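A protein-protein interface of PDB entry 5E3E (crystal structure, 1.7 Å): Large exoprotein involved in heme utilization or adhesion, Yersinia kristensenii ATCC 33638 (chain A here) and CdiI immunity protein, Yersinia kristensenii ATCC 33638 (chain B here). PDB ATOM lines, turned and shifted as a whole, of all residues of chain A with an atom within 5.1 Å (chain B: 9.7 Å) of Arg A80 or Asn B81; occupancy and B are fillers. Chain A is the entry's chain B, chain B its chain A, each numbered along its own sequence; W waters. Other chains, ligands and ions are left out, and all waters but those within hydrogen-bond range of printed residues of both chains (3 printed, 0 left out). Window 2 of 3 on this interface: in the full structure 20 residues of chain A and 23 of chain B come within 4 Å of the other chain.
NZ of Lys A26 sits at hydrogen-bond distance from O of Leu B70, at 3.0 Å. The backbone NH (N) of Lys A26 sits at hydrogen-bond distance from the backbone carbonyl oxygen (O) of Ser B76. O of Asn A24 lies within hydrogen-bond range of N of Tyr B78, 2.9 Å away. ND2 of Asn B81 sits close to NH2 of Arg A80 (3.5 Å).
OH of Tyr B77 is in hydrogen-bond range of OE2 of Glu B82, at 2.9 Å. The backbone carbonyl oxygen (O) of Val A20 sits close to the guanidinium group (NH2) of Arg A80, at 3.2 Å. The backbone carbonyl oxygen (O) of Ser A21 sits at hydrogen-bond distance from the guanidinium group (NH2) of Arg A80 (3.2 Å). The backbone carbonyl oxygen (O) of Gly A23 sits at hydrogen-bond distance from the guanidinium group (NH1) of Arg A80. The backbone carbonyl oxygen of Val A25 sits at hydrogen-bond distance from the guanidinium group of Arg A80, at 2.9 Å. O of Lys A26 lies within hydrogen-bond range of N of Arg A80.
Asn A24 touches Phe B22 (ND2 to CZ, 3.5 Å). Tyr B77 touches Asn A24 (CD1 to O, 3.6 Å). O of Ser B76 touches CA of Val A25 (3.0 Å). Tyr B78 touches Val A25. Lys A26 touches Asn B71 (CE to OD1, 3.9 Å). N of Lys A26 touches CB of Tyr B78, at 3.9 Å. Arg A80 touches Tyr B78.
Of the printed residues of chain B, Arg A80 touches Tyr B78 and Asn B81. Asn B81 touches one residue of chain A. No residue of chain B comes within 4 Å of Val A20. No residue of chain B comes within 4 Å of Gly A23. Ser A79 touches none of the printed residues of chain B. No residue of chain B comes within 4 Å of Gly A81. Printed residues of chain B within 4 Å of Asn A24: Phe B22, Tyr B77 and Tyr B78. Of the printed residues of chain A, Asn B71 touches Lys A26 (3.9 Å). Of the printed residues of chain B, Lys A26 touches Leu B70 (3.0 Å), Asn B71 (3.9 Å), Ser B76 (2.8 Å) and Tyr B78 (3.9 Å). Printed residues of chain A within 4 Å of Tyr B77: Asn A24. Trp B89 touches none of the printed residues of chain A. Ser A82 touches none of the printed residues of chain B. The nearest residue of chain B that does not touch Arg A80 is Ser B76 (6.9 Å). The nearest printed residue of chain A that does not touch Tyr B77 is Val A25 (4.7 Å).
Hydrophobic or aromatic side chains of chain B that line the printed part of chain A: Phe B22, Leu B70, Tyr B77 and Tyr B78. Of the 13 printed residues of chain A, 4 touch a printed residue of chain B. Printed residues of chain A that touch a printed residue of chain B: Asn A24, Val A25, Lys A26 and Arg A80. Hydrophobic or aromatic side chains of chain A that line the printed part of chain B: Val A25.
Water W1 lies within hydrogen-bond range of the side-chain hydroxyl of Ser A27 (2.6 Å), the side-chain amino group of Lys A26 (2.9 Å) and the side-chain hydroxyl of Ser B76 (3.3 Å). Water W3 bridges the side-chain amide nitrogen of Asn B81 (2.8 Å) and the backbone carbonyl oxygen of Gly A23 (3.5 Å). Water W2 lies within hydrogen-bond range of the side-chain amide nitrogen (ND2) of Asn A24 and the side-chain carboxylate (OE2) of Glu B82.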
ATOM      1  N   ARG A  19       5.340  22.597  23.036  1.00  0.00           N
ATOM      2  CA  ARG A  19       6.724  22.951  22.683  1.00  0.00           C
ATOM      3  C   ARG A  19       7.581  23.249  23.907  1.00  0.00           C
ATOM      4  O   ARG A  19       8.781  22.928  23.928  1.00  0.00           O
ATOM      5  CB  ARG A  19       6.738  24.153  21.769  1.00  0.00           C
ATOM      6  CG  ARG A  19       6.085  23.919  20.426  1.00  0.00           C
ATOM      7  CD  ARG A  19       6.043  25.219  19.662  1.00  0.00           C
ATOM      8  NE  ARG A  19       5.348  25.031  18.401  1.00  0.00           N
ATOM      9  CZ  ARG A  19       5.092  25.984  17.509  1.00  0.00           C
ATOM     10  NH1 ARG A  19       5.495  27.230  17.679  1.00  0.00           N
ATOM     11  NH2 ARG A  19       4.428  25.669  16.415  1.00  0.00           N
ATOM     12  N   VAL A  20       6.996  23.848  24.943  1.00  0.00           N
ATOM     13  CA  VAL A  20       7.770  24.184  26.136  1.00  0.00           C
ATOM     14  C   VAL A  20       7.811  23.078  27.186  1.00  0.00           C
ATOM     15  O   VAL A  20       8.348  23.291  28.269  1.00  0.00           O
ATOM     16  CB  VAL A  20       7.333  25.491  26.802  1.00  0.00           C
ATOM     17  CG1 VAL A  20       7.560  26.644  25.859  1.00  0.00           C
ATOM     18  CG2 VAL A  20       5.895  25.437  27.296  1.00  0.00           C
ATOM     19  N   SER A  21       7.219  21.921  26.925  1.00  0.00           N
ATOM     20  CA  SER A  21       7.330  20.818  27.894  1.00  0.00           C
ATOM     21  C   SER A  21       8.114  19.699  27.254  1.00  0.00           C
ATOM     22  O   SER A  21       9.276  19.465  27.595  1.00  0.00           O
ATOM     23  CB  SER A  21       5.946  20.391  28.381  1.00  0.00           C
ATOM     24  OG  SER A  21       5.090  20.153  27.296  1.00  0.00           O
ATOM     25  N   GLY A  23       9.106  19.709  24.018  1.00  0.00           N
ATOM     26  CA  GLY A  23      10.157  20.362  23.225  1.00  0.00           C
ATOM     27  C   GLY A  23      11.243  20.947  24.094  1.00  0.00           C
ATOM     28  O   GLY A  23      11.265  20.705  25.322  1.00  0.00           O
ATOM     29  N   ASN A  24      12.170  21.667  23.458  1.00  0.00           N
ATOM     30  CA  ASN A  24      13.407  22.096  24.124  1.00  0.00           C
ATOM     31  C   ASN A  24      13.671  23.621  24.035  1.00  0.00           C
ATOM     32  O   ASN A  24      14.849  24.100  24.041  1.00  0.00           O
ATOM     33  CB  ASN A  24      14.583  21.343  23.561  1.00  0.00           C
ATOM     34  CG  ASN A  24      14.762  21.593  22.085  1.00  0.00           C
ATOM     35  OD1 ASN A  24      13.957  22.298  21.482  1.00  0.00           O
ATOM     36  ND2 ASN A  24      15.826  21.031  21.486  1.00  0.00           N
ATOM     37  N   VAL A  25      12.583  24.368  23.907  1.00  0.00           N
ATOM     38  CA  VAL A  25      12.637  25.807  23.924  1.00  0.00           C
ATOM     39  C   VAL A  25      12.213  26.312  25.275  1.00  0.00           C
ATOM     40  O   VAL A  25      11.417  25.649  25.997  1.00  0.00           O
ATOM     41  CB  VAL A  25      11.751  26.479  22.828  1.00  0.00           C
ATOM     42  CG1 VAL A  25      12.361  26.268  21.457  1.00  0.00           C
ATOM     43  CG2 VAL A  25      10.304  26.000  22.911  1.00  0.00           C
ATOM     44  N   LYS A  26      12.711  27.485  25.634  1.00  0.00           N
ATOM     45  CA  LYS A  26      12.395  28.060  26.945  1.00  0.00           C
ATOM     46  C   LYS A  26      10.993  28.659  26.928  1.00  0.00           C
ATOM     47  O   LYS A  26      10.386  28.852  28.005  1.00  0.00           O
ATOM     48  CB  LYS A  26      13.393  29.143  27.382  1.00  0.00           C
ATOM     49  CG  LYS A  26      13.240  30.480  26.708  1.00  0.00           C
ATOM     50  CD  LYS A  26      13.842  31.589  27.507  1.00  0.00           C
ATOM     51  CE  LYS A  26      13.381  32.910  26.940  1.00  0.00           C
ATOM     52  NZ  LYS A  26      14.010  33.157  25.631  1.00  0.00           N
ATOM     53  N   SER A  27      10.558  29.045  25.733  1.00  0.00           N
ATOM     54  CA  SER A  27       9.265  29.719  25.527  1.00  0.00           C
ATOM     55  C   SER A  27       8.855  29.595  24.080  1.00  0.00           C
ATOM     56  O   SER A  27       9.673  29.300  23.202  1.00  0.00           O
ATOM     57  CB  SER A  27       9.296  31.188  25.937  1.00  0.00           C
ATOM     58  OG  SER A  27      10.002  31.997  25.038  1.00  0.00           O
ATOM     59  N   VAL A  78       3.963  31.434  25.906  1.00  0.00           N
ATOM     60  CA  VAL A  78       4.056  30.584  27.060  1.00  0.00           C
ATOM     61  C   VAL A  78       5.533  30.286  27.342  1.00  0.00           C
ATOM     62  O   VAL A  78       6.376  30.298  26.445  1.00  0.00           O
ATOM     63  CB  VAL A  78       3.260  29.273  26.903  1.00  0.00           C
ATOM     64  CG1 VAL A  78       1.772  29.587  26.714  1.00  0.00           C
ATOM     65  CG2 VAL A  78       3.799  28.418  25.770  1.00  0.00           C
ATOM     66  N   SER A  79       5.792  29.993  28.609  1.00  0.00           N
ATOM     67  CA  SER A  79       7.149  29.710  29.105  1.00  0.00           C
ATOM     68  C   SER A  79       7.229  28.389  29.876  1.00  0.00           C
ATOM     69  O   SER A  79       6.286  27.995  30.545  1.00  0.00           O
ATOM     70  CB  SER A  79       7.597  30.866  30.031  1.00  0.00           C
ATOM     71  OG  SER A  79       7.900  32.002  29.230  1.00  0.00           O
ATOM     72  N   ARG A  80       8.376  27.728  29.786  1.00  0.00           N
ATOM     73  CA  ARG A  80       8.616  26.486  30.508  1.00  0.00           C
ATOM     74  C   ARG A  80       8.343  26.635  31.994  1.00  0.00           C
ATOM     75  O   ARG A  80       8.642  27.661  32.593  1.00  0.00           O
ATOM     76  CB  ARG A  80      10.074  26.020  30.282  1.00  0.00           C
ATOM     77  CG  ARG A  80      10.336  24.601  30.724  1.00  0.00           C
ATOM     78  CD  ARG A  80      11.697  24.119  30.225  1.00  0.00           C
ATOM     79  NE  ARG A  80      11.645  23.996  28.778  1.00  0.00           N
ATOM     80  CZ  ARG A  80      11.363  22.867  28.128  1.00  0.00           C
ATOM     81  NH1 ARG A  80      11.309  22.877  26.804  1.00  0.00           N
ATOM     82  NH2 ARG A  80      11.141  21.732  28.792  1.00  0.00           N
ATOM     83  N   GLY A  81       7.728  25.625  32.583  1.00  0.00           N
ATOM     84  CA  GLY A  81       7.491  25.628  34.020  1.00  0.00           C
ATOM     85  C   GLY A  81       6.140  26.154  34.451  1.00  0.00           C
ATOM     86  O   GLY A  81       5.786  26.040  35.625  1.00  0.00           O
ATOM     87  N   SER A  82       5.360  26.703  33.522  1.00  0.00           N
ATOM     88  CA  SER A  82       4.080  27.294  33.846  1.00  0.00           C
ATOM     89  C   SER A  82       3.101  27.108  32.706  1.00  0.00           C
ATOM     90  O   SER A  82       3.518  26.973  31.574  1.00  0.00           O
ATOM     91  CB  SER A  82       4.284  28.776  34.058  1.00  0.00           C
ATOM     92  OG  SER A  82       3.079  29.393  34.389  1.00  0.00           O
ATOM     93  N   PHE B  22      15.034  26.757  15.733  1.00  0.00           N
ATOM     94  CA  PHE B  22      16.392  26.217  15.471  1.00  0.00           C
ATOM     95  C   PHE B  22      16.418  24.732  15.098  1.00  0.00           C
ATOM     96  O   PHE B  22      17.232  24.330  14.292  1.00  0.00           O
ATOM     97  CB  PHE B  22      17.355  26.518  16.620  1.00  0.00           C
ATOM     98  CG  PHE B  22      17.209  25.620  17.824  1.00  0.00           C
ATOM     99  CD1 PHE B  22      16.307  25.929  18.821  1.00  0.00           C
ATOM    100  CD2 PHE B  22      18.021  24.487  17.982  1.00  0.00           C
ATOM    101  CE1 PHE B  22      16.178  25.122  19.955  1.00  0.00           C
ATOM    102  CE2 PHE B  22      17.893  23.681  19.107  1.00  0.00           C
ATOM    103  CZ  PHE B  22      16.943  23.988  20.076  1.00  0.00           C
ATOM    104  N   GLN B  66      22.190  32.570  34.056  1.00  0.00           N
ATOM    105  CA  GLN B  66      21.073  31.997  33.285  1.00  0.00           C
ATOM    106  C   GLN B  66      20.065  33.053  32.888  1.00  0.00           C
ATOM    107  O   GLN B  66      19.542  33.025  31.800  1.00  0.00           O
ATOM    108  CB  GLN B  66      20.363  30.860  34.046  1.00  0.00           C
ATOM    109  CG  GLN B  66      19.304  30.113  33.254  1.00  0.00           C
ATOM    110  CD  GLN B  66      18.643  29.014  34.073  1.00  0.00           C
ATOM    111  OE1 GLN B  66      19.289  28.033  34.515  1.00  0.00           O
ATOM    112  NE2 GLN B  66      17.354  29.163  34.278  1.00  0.00           N
ATOM    113  N   LEU B  70      19.209  33.391  28.899  1.00  0.00           N
ATOM    114  CA  LEU B  70      17.836  33.054  28.530  1.00  0.00           C
ATOM    115  C   LEU B  70      16.899  34.232  28.383  1.00  0.00           C
ATOM    116  O   LEU B  70      16.095  34.234  27.466  1.00  0.00           O
ATOM    117  CB  LEU B  70      17.257  32.034  29.520  1.00  0.00           C
ATOM    118  CG  LEU B  70      17.821  30.624  29.474  1.00  0.00           C
ATOM    119  CD1 LEU B  70      17.099  29.763  30.488  1.00  0.00           C
ATOM    120  CD2 LEU B  70      17.730  29.951  28.102  1.00  0.00           C
ATOM    121  N   ASN B  71      16.958  35.206  29.283  1.00  0.00           N
ATOM    122  CA  ASN B  71      15.997  36.291  29.296  1.00  0.00           C
ATOM    123  C   ASN B  71      16.475  37.613  28.737  1.00  0.00           C
ATOM    124  O   ASN B  71      15.758  38.235  27.962  1.00  0.00           O
ATOM    125  CB  ASN B  71      15.460  36.465  30.703  1.00  0.00           C
ATOM    126  CG  ASN B  71      14.845  35.181  31.223  1.00  0.00           C
ATOM    127  OD1 ASN B  71      14.136  34.487  30.481  1.00  0.00           O
ATOM    128  ND2 ASN B  71      15.198  34.793  32.449  1.00  0.00           N
ATOM    129  N   SER B  76      16.469  31.083  22.769  1.00  0.00           N
ATOM    130  CA  SER B  76      15.223  30.233  22.780  1.00  0.00           C
ATOM    131  C   SER B  76      15.502  28.788  23.186  1.00  0.00           C
ATOM    132  O   SER B  76      14.591  28.086  23.623  1.00  0.00           O
ATOM    133  CB  SER B  76      14.549  30.204  21.398  1.00  0.00           C
ATOM    134  OG  SER B  76      14.130  31.498  21.022  1.00  0.00           O
ATOM    135  N   TYR B  77      16.752  28.337  23.075  1.00  0.00           N
ATOM    136  CA  TYR B  77      17.126  26.980  23.444  1.00  0.00           C
ATOM    137  C   TYR B  77      17.300  26.837  24.946  1.00  0.00           C
ATOM    138  O   TYR B  77      18.063  27.609  25.569  1.00  0.00           O
ATOM    139  CB  TYR B  77      18.408  26.594  22.713  1.00  0.00           C
ATOM    140  CG  TYR B  77      19.082  25.346  23.225  1.00  0.00           C
ATOM    141  CD1 TYR B  77      18.347  24.166  23.431  1.00  0.00           C
ATOM    142  CD2 TYR B  77      20.452  25.327  23.488  1.00  0.00           C
ATOM    143  CE1 TYR B  77      18.969  23.004  23.887  1.00  0.00           C
ATOM    144  CE2 TYR B  77      21.067  24.179  23.950  1.00  0.00           C
ATOM    145  CZ  TYR B  77      20.338  23.033  24.138  1.00  0.00           C
ATOM    146  OH  TYR B  77      21.002  21.880  24.583  1.00  0.00           O
ATOM    147  N   TYR B  78      16.506  25.935  25.550  1.00  0.00           N
ATOM    148  CA  TYR B  78      16.551  25.726  27.000  1.00  0.00           C
ATOM    149  C   TYR B  78      17.708  24.757  27.334  1.00  0.00           C
ATOM    150  O   TYR B  78      17.515  23.563  27.659  1.00  0.00           O
ATOM    151  CB  TYR B  78      15.213  25.214  27.516  1.00  0.00           C
ATOM    152  CG  TYR B  78      15.145  25.237  29.004  1.00  0.00           C
ATOM    153  CD1 TYR B  78      15.104  26.442  29.662  1.00  0.00           C
ATOM    154  CD2 TYR B  78      15.204  24.054  29.758  1.00  0.00           C
ATOM    155  CE1 TYR B  78      15.061  26.496  31.043  1.00  0.00           C
ATOM    156  CE2 TYR B  78      15.204  24.095  31.152  1.00  0.00           C
ATOM    157  CZ  TYR B  78      15.091  25.334  31.775  1.00  0.00           C
ATOM    158  OH  TYR B  78      15.075  25.461  33.139  1.00  0.00           O
ATOM    159  N   TYR B  79      18.921  25.286  27.226  1.00  0.00           N
ATOM    160  CA  TYR B  79      20.153  24.525  27.484  1.00  0.00           C
ATOM    161  C   TYR B  79      20.233  23.871  28.878  1.00  0.00           C
ATOM    162  O   TYR B  79      20.888  22.833  29.006  1.00  0.00           O
ATOM    163  CB  TYR B  79      21.403  25.387  27.191  1.00  0.00           C
ATOM    164  CG  TYR B  79      21.521  26.562  28.117  1.00  0.00           C
ATOM    165  CD1 TYR B  79      22.099  26.442  29.386  1.00  0.00           C
ATOM    166  CD2 TYR B  79      21.010  27.787  27.735  1.00  0.00           C
ATOM    167  CE1 TYR B  79      22.125  27.537  30.275  1.00  0.00           C
ATOM    168  CE2 TYR B  79      21.025  28.878  28.603  1.00  0.00           C
ATOM    169  CZ  TYR B  79      21.607  28.748  29.866  1.00  0.00           C
ATOM    170  OH  TYR B  79      21.661  29.846  30.737  1.00  0.00           O
ATOM    171  N   PRO B  80      19.516  24.404  29.915  1.00  0.00           N
ATOM    172  CA  PRO B  80      19.656  23.691  31.208  1.00  0.00           C
ATOM    173  C   PRO B  80      19.168  22.224  31.168  1.00  0.00           C
ATOM    174  O   PRO B  80      19.536  21.429  32.037  1.00  0.00           O
ATOM    175  CB  PRO B  80      18.836  24.558  32.174  1.00  0.00           C
ATOM    176  CG  PRO B  80      18.948  25.906  31.601  1.00  0.00           C
ATOM    177  CD  PRO B  80      18.789  25.668  30.129  1.00  0.00           C
ATOM    178  N   ASN B  81      18.416  21.825  30.154  1.00  0.00           N
ATOM    179  CA  ASN B  81      18.006  20.419  30.112  1.00  0.00           C
ATOM    180  C   ASN B  81      19.114  19.508  29.654  1.00  0.00           C
ATOM    181  O   ASN B  81      19.037  18.300  29.896  1.00  0.00           O
ATOM    182  CB  ASN B  81      16.673  20.241  29.378  1.00  0.00           C
ATOM    183  CG  ASN B  81      15.469  20.490  30.315  1.00  0.00           C
ATOM    184  OD1 ASN B  81      15.586  20.439  31.560  1.00  0.00           O
ATOM    185  ND2 ASN B  81      14.320  20.753  29.736  1.00  0.00           N
ATOM    186  N   GLU B  82      20.153  20.067  29.036  1.00  0.00           N
ATOM    187  CA  GLU B  82      21.338  19.311  28.638  1.00  0.00           C
ATOM    188  C   GLU B  82      22.592  19.660  29.425  1.00  0.00           C
ATOM    189  O   GLU B  82      23.589  18.972  29.264  1.00  0.00           O
ATOM    190  CB  GLU B  82      21.630  19.517  27.162  1.00  0.00           C
ATOM    191  CG  GLU B  82      20.798  18.612  26.262  1.00  0.00           C
ATOM    192  CD  GLU B  82      19.364  19.014  26.203  1.00  0.00           C
ATOM    193  OE1 GLU B  82      18.523  18.335  26.816  1.00  0.00           O
ATOM    194  OE2 GLU B  82      19.069  20.020  25.556  1.00  0.00           O
ATOM    195  N   TRP B  83      22.580  20.755  30.212  1.00  0.00           N
ATOM    196  CA  TRP B  83      23.810  21.302  30.798  1.00  0.00           C
ATOM    197  C   TRP B  83      23.579  21.670  32.245  1.00  0.00           C
ATOM    198  O   TRP B  83      22.572  22.270  32.560  1.00  0.00           O
ATOM    199  CB  TRP B  83      24.321  22.534  30.022  1.00  0.00           C
ATOM    200  CG  TRP B  83      24.761  22.129  28.646  1.00  0.00           C
ATOM    201  CD1 TRP B  83      24.005  22.095  27.524  1.00  0.00           C
ATOM    202  CD2 TRP B  83      26.016  21.542  28.313  1.00  0.00           C
ATOM    203  NE1 TRP B  83      24.736  21.529  26.466  1.00  0.00           N
ATOM    204  CE2 TRP B  83      25.979  21.216  26.936  1.00  0.00           C
ATOM    205  CE3 TRP B  83      27.181  21.265  29.043  1.00  0.00           C
ATOM    206  CZ2 TRP B  83      27.069  20.647  26.282  1.00  0.00           C
ATOM    207  CZ3 TRP B  83      28.258  20.706  28.383  1.00  0.00           C
ATOM    208  CH2 TRP B  83      28.184  20.380  27.033  1.00  0.00           C
ATOM    209  N   SER B  84      24.532  21.311  33.105  1.00  0.00           N
ATOM    210  CA  SER B  84      24.395  21.468  34.561  1.00  0.00           C
ATOM    211  C   SER B  84      24.451  22.924  34.978  1.00  0.00           C
ATOM    212  O   SER B  84      23.997  23.243  36.072  1.00  0.00           O
ATOM    213  CB  SER B  84      25.507  20.731  35.338  1.00  0.00           C
ATOM    214  OG  SER B  84      26.811  21.296  35.072  1.00  0.00           O
ATOM    215  N   SER B  85      25.023  23.776  34.137  1.00  0.00           N
ATOM    216  CA  SER B  85      25.194  25.197  34.468  1.00  0.00           C
ATOM    217  C   SER B  85      25.356  25.998  33.198  1.00  0.00           C
ATOM    218  O   SER B  85      25.745  25.471  32.141  1.00  0.00           O
ATOM    219  CB  SER B  85      26.406  25.444  35.391  1.00  0.00           C
ATOM    220  OG  SER B  85      27.636  25.295  34.659  1.00  0.00           O
ATOM    221  N   SER B  86      25.121  27.295  33.315  1.00  0.00           N
ATOM    222  CA  SER B  86      25.315  28.225  32.218  1.00  0.00           C
ATOM    223  C   SER B  86      26.810  28.340  31.858  1.00  0.00           C
ATOM    224  O   SER B  86      27.159  28.407  30.681  1.00  0.00           O
ATOM    225  CB  SER B  86      24.704  29.580  32.550  1.00  0.00           C
ATOM    226  OG  SER B  86      23.304  29.459  32.814  1.00  0.00           O
ATOM    227  N   TRP B  89      27.690  25.377  29.583  1.00  0.00           N
ATOM    228  CA  TRP B  89      27.181  25.498  28.223  1.00  0.00           C
ATOM    229  C   TRP B  89      28.032  26.513  27.467  1.00  0.00           C
ATOM    230  O   TRP B  89      28.394  26.270  26.321  1.00  0.00           O
ATOM    231  CB  TRP B  89      25.712  25.907  28.161  1.00  0.00           C
ATOM    232  CG  TRP B  89      25.210  25.854  26.764  1.00  0.00           C
ATOM    233  CD1 TRP B  89      25.372  24.806  25.890  1.00  0.00           C
ATOM    234  CD2 TRP B  89      24.550  26.884  26.027  1.00  0.00           C
ATOM    235  NE1 TRP B  89      24.832  25.114  24.669  1.00  0.00           N
ATOM    236  CE2 TRP B  89      24.308  26.382  24.733  1.00  0.00           C
ATOM    237  CE3 TRP B  89      24.077  28.159  26.357  1.00  0.00           C
ATOM    238  CZ2 TRP B  89      23.647  27.115  23.764  1.00  0.00           C
ATOM    239  CZ3 TRP B  89      23.439  28.883  25.390  1.00  0.00           C
ATOM    240  CH2 TRP B  89      23.214  28.369  24.123  1.00  0.00           C
HETATM  241  O   HOH W   1      12.185  31.893  23.710  1.00  0.00           O
HETATM  242  O   HOH W   2      17.147  19.257  23.395  1.00  0.00           O
HETATM  243  O   HOH W   3      14.307  20.268  26.971  1.00  0.00           O
